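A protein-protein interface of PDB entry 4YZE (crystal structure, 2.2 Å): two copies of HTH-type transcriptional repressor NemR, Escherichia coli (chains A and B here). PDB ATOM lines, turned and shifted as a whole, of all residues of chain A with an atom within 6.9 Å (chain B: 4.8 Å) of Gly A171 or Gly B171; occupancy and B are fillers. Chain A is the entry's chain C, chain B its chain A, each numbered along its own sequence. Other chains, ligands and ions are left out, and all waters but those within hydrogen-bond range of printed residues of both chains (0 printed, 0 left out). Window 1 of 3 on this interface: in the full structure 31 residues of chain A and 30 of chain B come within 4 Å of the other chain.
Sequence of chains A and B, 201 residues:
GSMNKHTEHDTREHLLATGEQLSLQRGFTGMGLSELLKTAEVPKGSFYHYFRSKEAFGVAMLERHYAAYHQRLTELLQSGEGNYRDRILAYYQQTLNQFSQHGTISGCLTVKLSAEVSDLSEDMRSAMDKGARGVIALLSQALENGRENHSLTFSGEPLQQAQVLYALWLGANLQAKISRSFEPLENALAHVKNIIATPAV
Of the 9 printed residues of chain B, 6 touch a printed residue of chain A.
Printed residues of chain B that touch a printed residue of chain A: Ala B167, Leu B170, Gly B171, Ala B172, Leu B174 and Gln B175.
Of the 14 printed residues of chain A, 8 touch a printed residue of chain B.
Hydrophobic or aromatic side chains of chain A that line the printed part of chain B: Tyr A166, Ala A167, Leu A168, Leu A170 and Leu A174.
Along chain A the printed residues that touch a printed residue of chain B span positions 166 to 175.
Among the printed residues, no Asp or Glu carboxylate lies within 4 Å of a Lys or Arg side-chain nitrogen of the other chain.
Printed residues of chain B within 4 Å of Tyr A166: Gln B175.
Of chain B, only Ala B167 (3.2 Å) and Gly B171 (3.7 Å) come within 4 Å of Gly A171.
Of the printed residues of chain B, Gln A175 touches Leu B170.
Pro A184 touches none of the printed residues of chain B.
Gly B171 touches just these residues of chain A: Ala A167, Leu A170 and Gly A171.
The nearest residue of chain A that does not touch Gly B171 is Leu A168 (5.3 Å).
Ala A167 touches Gln B175, but with the chains exchanged Gln A175 does not touch Ala B167 (5.4 Å).
Leu A170 touches Gly B171, but with the chains exchanged Gly A171 does not touch Leu B170 (4.04 Å).
Leu A174 touches Leu B170, but with the chains exchanged Leu A170 does not touch Leu B174 (4.05 Å).
Leu A174 touches its own counterpart, Leu B174.
Among the printed residues, merely in contact across the chains: Tyr A166 with Gln B175 (3.3 Å), Ala A167 with Ala B167 (3.8 Å), Ala A167 with Gly B171 (3.3 Å), Ala A167 with Ala B172 (3.9 Å), Ala A167 with Gln B175 (3.9 Å), Leu A168 with Ala B167 (3.8 Å), Leu A170 with Gly B171 (3.9 Å), Gly A171 with Ala B167 (3.2 Å), Gly A171 with Gly B171 (3.7 Å), Ala A172 with Ala B167 (3.8 Å), Leu A174 with Leu B170 (3.7 Å), Leu A174 with Leu B174 (3.7 Å) and Gln A175 with Leu B170 (3.99 Å).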
ATOM      1  N   TYR A 166     -31.682  -1.678  -9.718  1.00  0.00           N
ATOM      2  CA  TYR A 166     -31.038  -0.804  -8.743  1.00  0.00           C
ATOM      3  C   TYR A 166     -29.611  -0.504  -9.183  1.00  0.00           C
ATOM      4  O   TYR A 166     -29.194   0.641  -9.204  1.00  0.00           O
ATOM      5  CB  TYR A 166     -31.051  -1.441  -7.343  1.00  0.00           C
ATOM      6  CG  TYR A 166     -30.394  -0.534  -6.325  1.00  0.00           C
ATOM      7  CD1 TYR A 166     -30.992   0.662  -5.958  1.00  0.00           C
ATOM      8  CD2 TYR A 166     -29.173  -0.860  -5.754  1.00  0.00           C
ATOM      9  CE1 TYR A 166     -30.391   1.522  -5.039  1.00  0.00           C
ATOM     10  CE2 TYR A 166     -28.567  -0.017  -4.827  1.00  0.00           C
ATOM     11  CZ  TYR A 166     -29.189   1.174  -4.473  1.00  0.00           C
ATOM     12  OH  TYR A 166     -28.592   2.023  -3.561  1.00  0.00           O
ATOM     13  N   ALA A 167     -28.855  -1.535  -9.544  1.00  0.00           N
ATOM     14  CA  ALA A 167     -27.467  -1.320  -9.972  1.00  0.00           C
ATOM     15  C   ALA A 167     -27.371  -0.447 -11.232  1.00  0.00           C
ATOM     16  O   ALA A 167     -26.432   0.349 -11.390  1.00  0.00           O
ATOM     17  CB  ALA A 167     -26.752  -2.670 -10.178  1.00  0.00           C
ATOM     18  N   LEU A 168     -28.339  -0.581 -12.129  1.00  0.00           N
ATOM     19  CA  LEU A 168     -28.334   0.217 -13.352  1.00  0.00           C
ATOM     20  C   LEU A 168     -28.578   1.674 -13.009  1.00  0.00           C
ATOM     21  O   LEU A 168     -27.935   2.569 -13.552  1.00  0.00           O
ATOM     22  CB  LEU A 168     -29.470  -0.238 -14.288  1.00  0.00           C
ATOM     23  CG  LEU A 168     -29.381  -0.188 -15.814  1.00  0.00           C
ATOM     24  CD1 LEU A 168     -30.808  -0.140 -16.451  1.00  0.00           C
ATOM     25  CD2 LEU A 168     -28.501   0.899 -16.351  1.00  0.00           C
ATOM     26  N   TRP A 169     -29.566   1.912 -12.159  1.00  0.00           N
ATOM     27  CA  TRP A 169     -29.897   3.266 -11.744  1.00  0.00           C
ATOM     28  C   TRP A 169     -28.660   3.955 -11.135  1.00  0.00           C
ATOM     29  O   TRP A 169     -28.382   5.119 -11.411  1.00  0.00           O
ATOM     30  CB  TRP A 169     -31.014   3.173 -10.708  1.00  0.00           C
ATOM     31  CG  TRP A 169     -31.520   4.484 -10.170  1.00  0.00           C
ATOM     32  CD1 TRP A 169     -32.515   5.253 -10.693  1.00  0.00           C
ATOM     33  CD2 TRP A 169     -31.078   5.151  -8.983  1.00  0.00           C
ATOM     34  NE1 TRP A 169     -32.711   6.363  -9.914  1.00  0.00           N
ATOM     35  CE2 TRP A 169     -31.843   6.322  -8.850  1.00  0.00           C
ATOM     36  CE3 TRP A 169     -30.110   4.865  -8.012  1.00  0.00           C
ATOM     37  CZ2 TRP A 169     -31.664   7.226  -7.791  1.00  0.00           C
ATOM     38  CZ3 TRP A 169     -29.936   5.754  -6.957  1.00  0.00           C
ATOM     39  CH2 TRP A 169     -30.708   6.923  -6.857  1.00  0.00           C
ATOM     40  N   LEU A 170     -27.927   3.206 -10.314  1.00  0.00           N
ATOM     41  CA  LEU A 170     -26.779   3.728  -9.578  1.00  0.00           C
ATOM     42  C   LEU A 170     -25.652   4.019 -10.558  1.00  0.00           C
ATOM     43  O   LEU A 170     -25.090   5.104 -10.556  1.00  0.00           O
ATOM     44  CB  LEU A 170     -26.336   2.678  -8.552  1.00  0.00           C
ATOM     45  CG  LEU A 170     -25.796   3.034  -7.172  1.00  0.00           C
ATOM     46  CD1 LEU A 170     -26.782   3.868  -6.328  1.00  0.00           C
ATOM     47  CD2 LEU A 170     -25.415   1.731  -6.451  1.00  0.00           C
ATOM     48  N   GLY A 171     -25.355   3.057 -11.429  1.00  0.00           N
ATOM     49  CA  GLY A 171     -24.313   3.218 -12.429  1.00  0.00           C
ATOM     50  C   GLY A 171     -24.644   4.331 -13.403  1.00  0.00           C
ATOM     51  O   GLY A 171     -23.756   5.106 -13.776  1.00  0.00           O
ATOM     52  N   ALA A 172     -25.913   4.435 -13.808  1.00  0.00           N
ATOM     53  CA  ALA A 172     -26.296   5.464 -14.783  1.00  0.00           C
ATOM     54  C   ALA A 172     -26.187   6.858 -14.152  1.00  0.00           C
ATOM     55  O   ALA A 172     -25.682   7.804 -14.778  1.00  0.00           O
ATOM     56  CB  ALA A 172     -27.709   5.202 -15.357  1.00  0.00           C
ATOM     57  N   ASN A 173     -26.645   6.983 -12.907  1.00  0.00           N
ATOM     58  CA  ASN A 173     -26.451   8.244 -12.173  1.00  0.00           C
ATOM     59  C   ASN A 173     -24.988   8.651 -12.077  1.00  0.00           C
ATOM     60  O   ASN A 173     -24.656   9.796 -12.296  1.00  0.00           O
ATOM     61  CB  ASN A 173     -27.070   8.167 -10.776  1.00  0.00           C
ATOM     62  CG  ASN A 173     -28.544   8.508 -10.782  1.00  0.00           C
ATOM     63  OD1 ASN A 173     -28.917   9.685 -10.815  1.00  0.00           O
ATOM     64  ND2 ASN A 173     -29.392   7.486 -10.760  1.00  0.00           N
ATOM     65  N   LEU A 174     -24.109   7.708 -11.756  1.00  0.00           N
ATOM     66  CA  LEU A 174     -22.683   8.010 -11.669  1.00  0.00           C
ATOM     67  C   LEU A 174     -22.152   8.449 -13.014  1.00  0.00           C
ATOM     68  O   LEU A 174     -21.415   9.429 -13.105  1.00  0.00           O
ATOM     69  CB  LEU A 174     -21.889   6.786 -11.229  1.00  0.00           C
ATOM     70  CG  LEU A 174     -21.418   6.722  -9.795  1.00  0.00           C
ATOM     71  CD1 LEU A 174     -20.337   5.693  -9.705  1.00  0.00           C
ATOM     72  CD2 LEU A 174     -20.905   8.097  -9.401  1.00  0.00           C
ATOM     73  N   GLN A 175     -22.520   7.707 -14.059  1.00  0.00           N
ATOM     74  CA  GLN A 175     -22.068   8.029 -15.399  1.00  0.00           C
ATOM     75  C   GLN A 175     -22.600   9.394 -15.844  1.00  0.00           C
ATOM     76  O   GLN A 175     -21.908  10.155 -16.531  1.00  0.00           O
ATOM     77  CB  GLN A 175     -22.475   6.913 -16.379  1.00  0.00           C
ATOM     78  CG  GLN A 175     -21.752   6.971 -17.719  1.00  0.00           C
ATOM     79  CD  GLN A 175     -20.283   7.384 -17.586  1.00  0.00           C
ATOM     80  OE1 GLN A 175     -19.586   6.971 -16.649  1.00  0.00           O
ATOM     81  NE2 GLN A 175     -19.808   8.201 -18.526  1.00  0.00           N
ATOM     82  N   ALA A 176     -23.827   9.717 -15.435  1.00  0.00           N
ATOM     83  CA  ALA A 176     -24.392  11.037 -15.752  1.00  0.00           C
ATOM     84  C   ALA A 176     -23.601  12.142 -15.062  1.00  0.00           C
ATOM     85  O   ALA A 176     -23.429  13.241 -15.597  1.00  0.00           O
ATOM     86  CB  ALA A 176     -25.846  11.088 -15.319  1.00  0.00           C
ATOM     87  N   LYS A 177     -23.147  11.845 -13.848  1.00  0.00           N
ATOM     88  CA  LYS A 177     -22.451  12.825 -13.020  1.00  0.00           C
ATOM     89  C   LYS A 177     -21.076  13.063 -13.615  1.00  0.00           C
ATOM     90  O   LYS A 177     -20.630  14.207 -13.750  1.00  0.00           O
ATOM     91  CB  LYS A 177     -22.327  12.265 -11.595  1.00  0.00           C
ATOM     92  CG  LYS A 177     -21.855  13.240 -10.535  1.00  0.00           C
ATOM     93  CD  LYS A 177     -21.543  12.479  -9.241  1.00  0.00           C
ATOM     94  CE  LYS A 177     -20.917  13.362  -8.163  1.00  0.00           C
ATOM     95  NZ  LYS A 177     -20.473  12.576  -6.963  1.00  0.00           N
ATOM     96  N   PRO A 184     -26.865   8.952 -20.094  1.00  0.00           N
ATOM     97  CA  PRO A 184     -26.857   7.622 -19.463  1.00  0.00           C
ATOM     98  C   PRO A 184     -28.181   7.274 -18.811  1.00  0.00           C
ATOM     99  O   PRO A 184     -28.550   6.090 -18.790  1.00  0.00           O
ATOM    100  CB  PRO A 184     -25.758   7.741 -18.396  1.00  0.00           C
ATOM    101  CG  PRO A 184     -24.801   8.809 -18.978  1.00  0.00           C
ATOM    102  CD  PRO A 184     -25.721   9.786 -19.654  1.00  0.00           C
ATOM    103  N   LEU A 185     -28.894   8.278 -18.306  1.00  0.00           N
ATOM    104  CA  LEU A 185     -30.196   8.039 -17.677  1.00  0.00           C
ATOM    105  C   LEU A 185     -31.281   7.728 -18.714  1.00  0.00           C
ATOM    106  O   LEU A 185     -32.052   6.769 -18.550  1.00  0.00           O
ATOM    107  CB  LEU A 185     -30.611   9.232 -16.803  1.00  0.00           C
ATOM    108  CG  LEU A 185     -29.652   9.534 -15.647  1.00  0.00           C
ATOM    109  CD1 LEU A 185     -29.940  10.886 -14.959  1.00  0.00           C
ATOM    110  CD2 LEU A 185     -29.673   8.410 -14.636  1.00  0.00           C
ATOM    111  N   ALA B 167     -22.885   0.966 -17.360  1.00  0.00           N
ATOM    112  CA  ALA B 167     -23.590   1.495 -16.189  1.00  0.00           C
ATOM    113  C   ALA B 167     -23.840   0.354 -15.209  1.00  0.00           C
ATOM    114  O   ALA B 167     -23.684   0.509 -13.998  1.00  0.00           O
ATOM    115  CB  ALA B 167     -24.880   2.125 -16.591  1.00  0.00           C
ATOM    116  N   LEU B 168     -24.201  -0.811 -15.741  1.00  0.00           N
ATOM    117  CA  LEU B 168     -24.490  -1.967 -14.880  1.00  0.00           C
ATOM    118  C   LEU B 168     -23.257  -2.412 -14.094  1.00  0.00           C
ATOM    119  O   LEU B 168     -23.327  -2.689 -12.882  1.00  0.00           O
ATOM    120  CB  LEU B 168     -25.002  -3.129 -15.736  1.00  0.00           C
ATOM    121  CG  LEU B 168     -25.917  -4.237 -15.209  1.00  0.00           C
ATOM    122  CD1 LEU B 168     -25.624  -5.565 -15.908  1.00  0.00           C
ATOM    123  CD2 LEU B 168     -25.888  -4.414 -13.727  1.00  0.00           C
ATOM    124  N   TRP B 169     -22.140  -2.521 -14.803  1.00  0.00           N
ATOM    125  CA  TRP B 169     -20.855  -2.887 -14.211  1.00  0.00           C
ATOM    126  C   TRP B 169     -20.446  -1.912 -13.101  1.00  0.00           C
ATOM    127  O   TRP B 169     -19.966  -2.320 -12.042  1.00  0.00           O
ATOM    128  CB  TRP B 169     -19.805  -2.876 -15.332  1.00  0.00           C
ATOM    129  CG  TRP B 169     -18.387  -3.106 -14.904  1.00  0.00           C
ATOM    130  CD1 TRP B 169     -17.739  -4.306 -14.816  1.00  0.00           C
ATOM    131  CD2 TRP B 169     -17.419  -2.101 -14.544  1.00  0.00           C
ATOM    132  NE1 TRP B 169     -16.437  -4.111 -14.410  1.00  0.00           N
ATOM    133  CE2 TRP B 169     -16.217  -2.770 -14.234  1.00  0.00           C
ATOM    134  CE3 TRP B 169     -17.455  -0.706 -14.457  1.00  0.00           C
ATOM    135  CZ2 TRP B 169     -15.054  -2.085 -13.833  1.00  0.00           C
ATOM    136  CZ3 TRP B 169     -16.303  -0.029 -14.055  1.00  0.00           C
ATOM    137  CH2 TRP B 169     -15.120  -0.723 -13.749  1.00  0.00           C
ATOM    138  N   LEU B 170     -20.652  -0.624 -13.358  1.00  0.00           N
ATOM    139  CA  LEU B 170     -20.309   0.449 -12.426  1.00  0.00           C
ATOM    140  C   LEU B 170     -21.177   0.340 -11.178  1.00  0.00           C
ATOM    141  O   LEU B 170     -20.673   0.338 -10.040  1.00  0.00           O
ATOM    142  CB  LEU B 170     -20.503   1.821 -13.140  1.00  0.00           C
ATOM    143  CG  LEU B 170     -19.358   2.835 -13.210  1.00  0.00           C
ATOM    144  CD1 LEU B 170     -19.837   4.134 -13.851  1.00  0.00           C
ATOM    145  CD2 LEU B 170     -18.773   3.133 -11.838  1.00  0.00           C
ATOM    146  N   GLY B 171     -22.485   0.198 -11.374  1.00  0.00           N
ATOM    147  CA  GLY B 171     -23.398   0.178 -10.235  1.00  0.00           C
ATOM    148  C   GLY B 171     -23.228  -1.089  -9.410  1.00  0.00           C
ATOM    149  O   GLY B 171     -23.354  -1.094  -8.172  1.00  0.00           O
ATOM    150  N   ALA B 172     -22.904  -2.180 -10.083  1.00  0.00           N
ATOM    151  CA  ALA B 172     -22.800  -3.446  -9.366  1.00  0.00           C
ATOM    152  C   ALA B 172     -21.556  -3.429  -8.505  1.00  0.00           C
ATOM    153  O   ALA B 172     -21.565  -3.956  -7.392  1.00  0.00           O
ATOM    154  CB  ALA B 172     -22.777  -4.656 -10.338  1.00  0.00           C
ATOM    155  N   ASN B 173     -20.481  -2.863  -9.052  1.00  0.00           N
ATOM    156  CA  ASN B 173     -19.239  -2.679  -8.299  1.00  0.00           C
ATOM    157  C   ASN B 173     -19.432  -1.807  -7.066  1.00  0.00           C
ATOM    158  O   ASN B 173     -18.934  -2.119  -5.980  1.00  0.00           O
ATOM    159  CB  ASN B 173     -18.133  -2.104  -9.205  1.00  0.00           C
ATOM    160  CG  ASN B 173     -17.348  -3.207  -9.919  1.00  0.00           C
ATOM    161  OD1 ASN B 173     -16.641  -3.986  -9.271  1.00  0.00           O
ATOM    162  ND2 ASN B 173     -17.484  -3.291 -11.249  1.00  0.00           N
ATOM    163  N   LEU B 174     -20.163  -0.718  -7.249  1.00  0.00           N
ATOM    164  CA  LEU B 174     -20.433   0.218  -6.176  1.00  0.00           C
ATOM    165  C   LEU B 174     -21.133  -0.533  -5.075  1.00  0.00           C
ATOM    166  O   LEU B 174     -20.726  -0.515  -3.909  1.00  0.00           O
ATOM    167  CB  LEU B 174     -21.346   1.339  -6.675  1.00  0.00           C
ATOM    168  CG  LEU B 174     -20.744   2.738  -6.742  1.00  0.00           C
ATOM    169  CD1 LEU B 174     -21.830   3.795  -6.875  1.00  0.00           C
ATOM    170  CD2 LEU B 174     -19.918   2.990  -5.522  1.00  0.00           C
ATOM    171  N   GLN B 175     -22.187  -1.223  -5.473  1.00  0.00           N
ATOM    172  CA  GLN B 175     -22.992  -1.989  -4.552  1.00  0.00           C
ATOM    173  C   GLN B 175     -22.231  -3.144  -3.919  1.00  0.00           C
ATOM    174  O   GLN B 175     -22.480  -3.482  -2.765  1.00  0.00           O
ATOM    175  CB  GLN B 175     -24.191  -2.539  -5.303  1.00  0.00           C
ATOM    176  CG  GLN B 175     -25.271  -3.024  -4.406  1.00  0.00           C
ATOM    177  CD  GLN B 175     -26.557  -3.196  -5.144  1.00  0.00           C
ATOM    178  OE1 GLN B 175     -26.661  -2.856  -6.326  1.00  0.00           O
ATOM    179  NE2 GLN B 175     -27.554  -3.733  -4.460  1.00  0.00           N
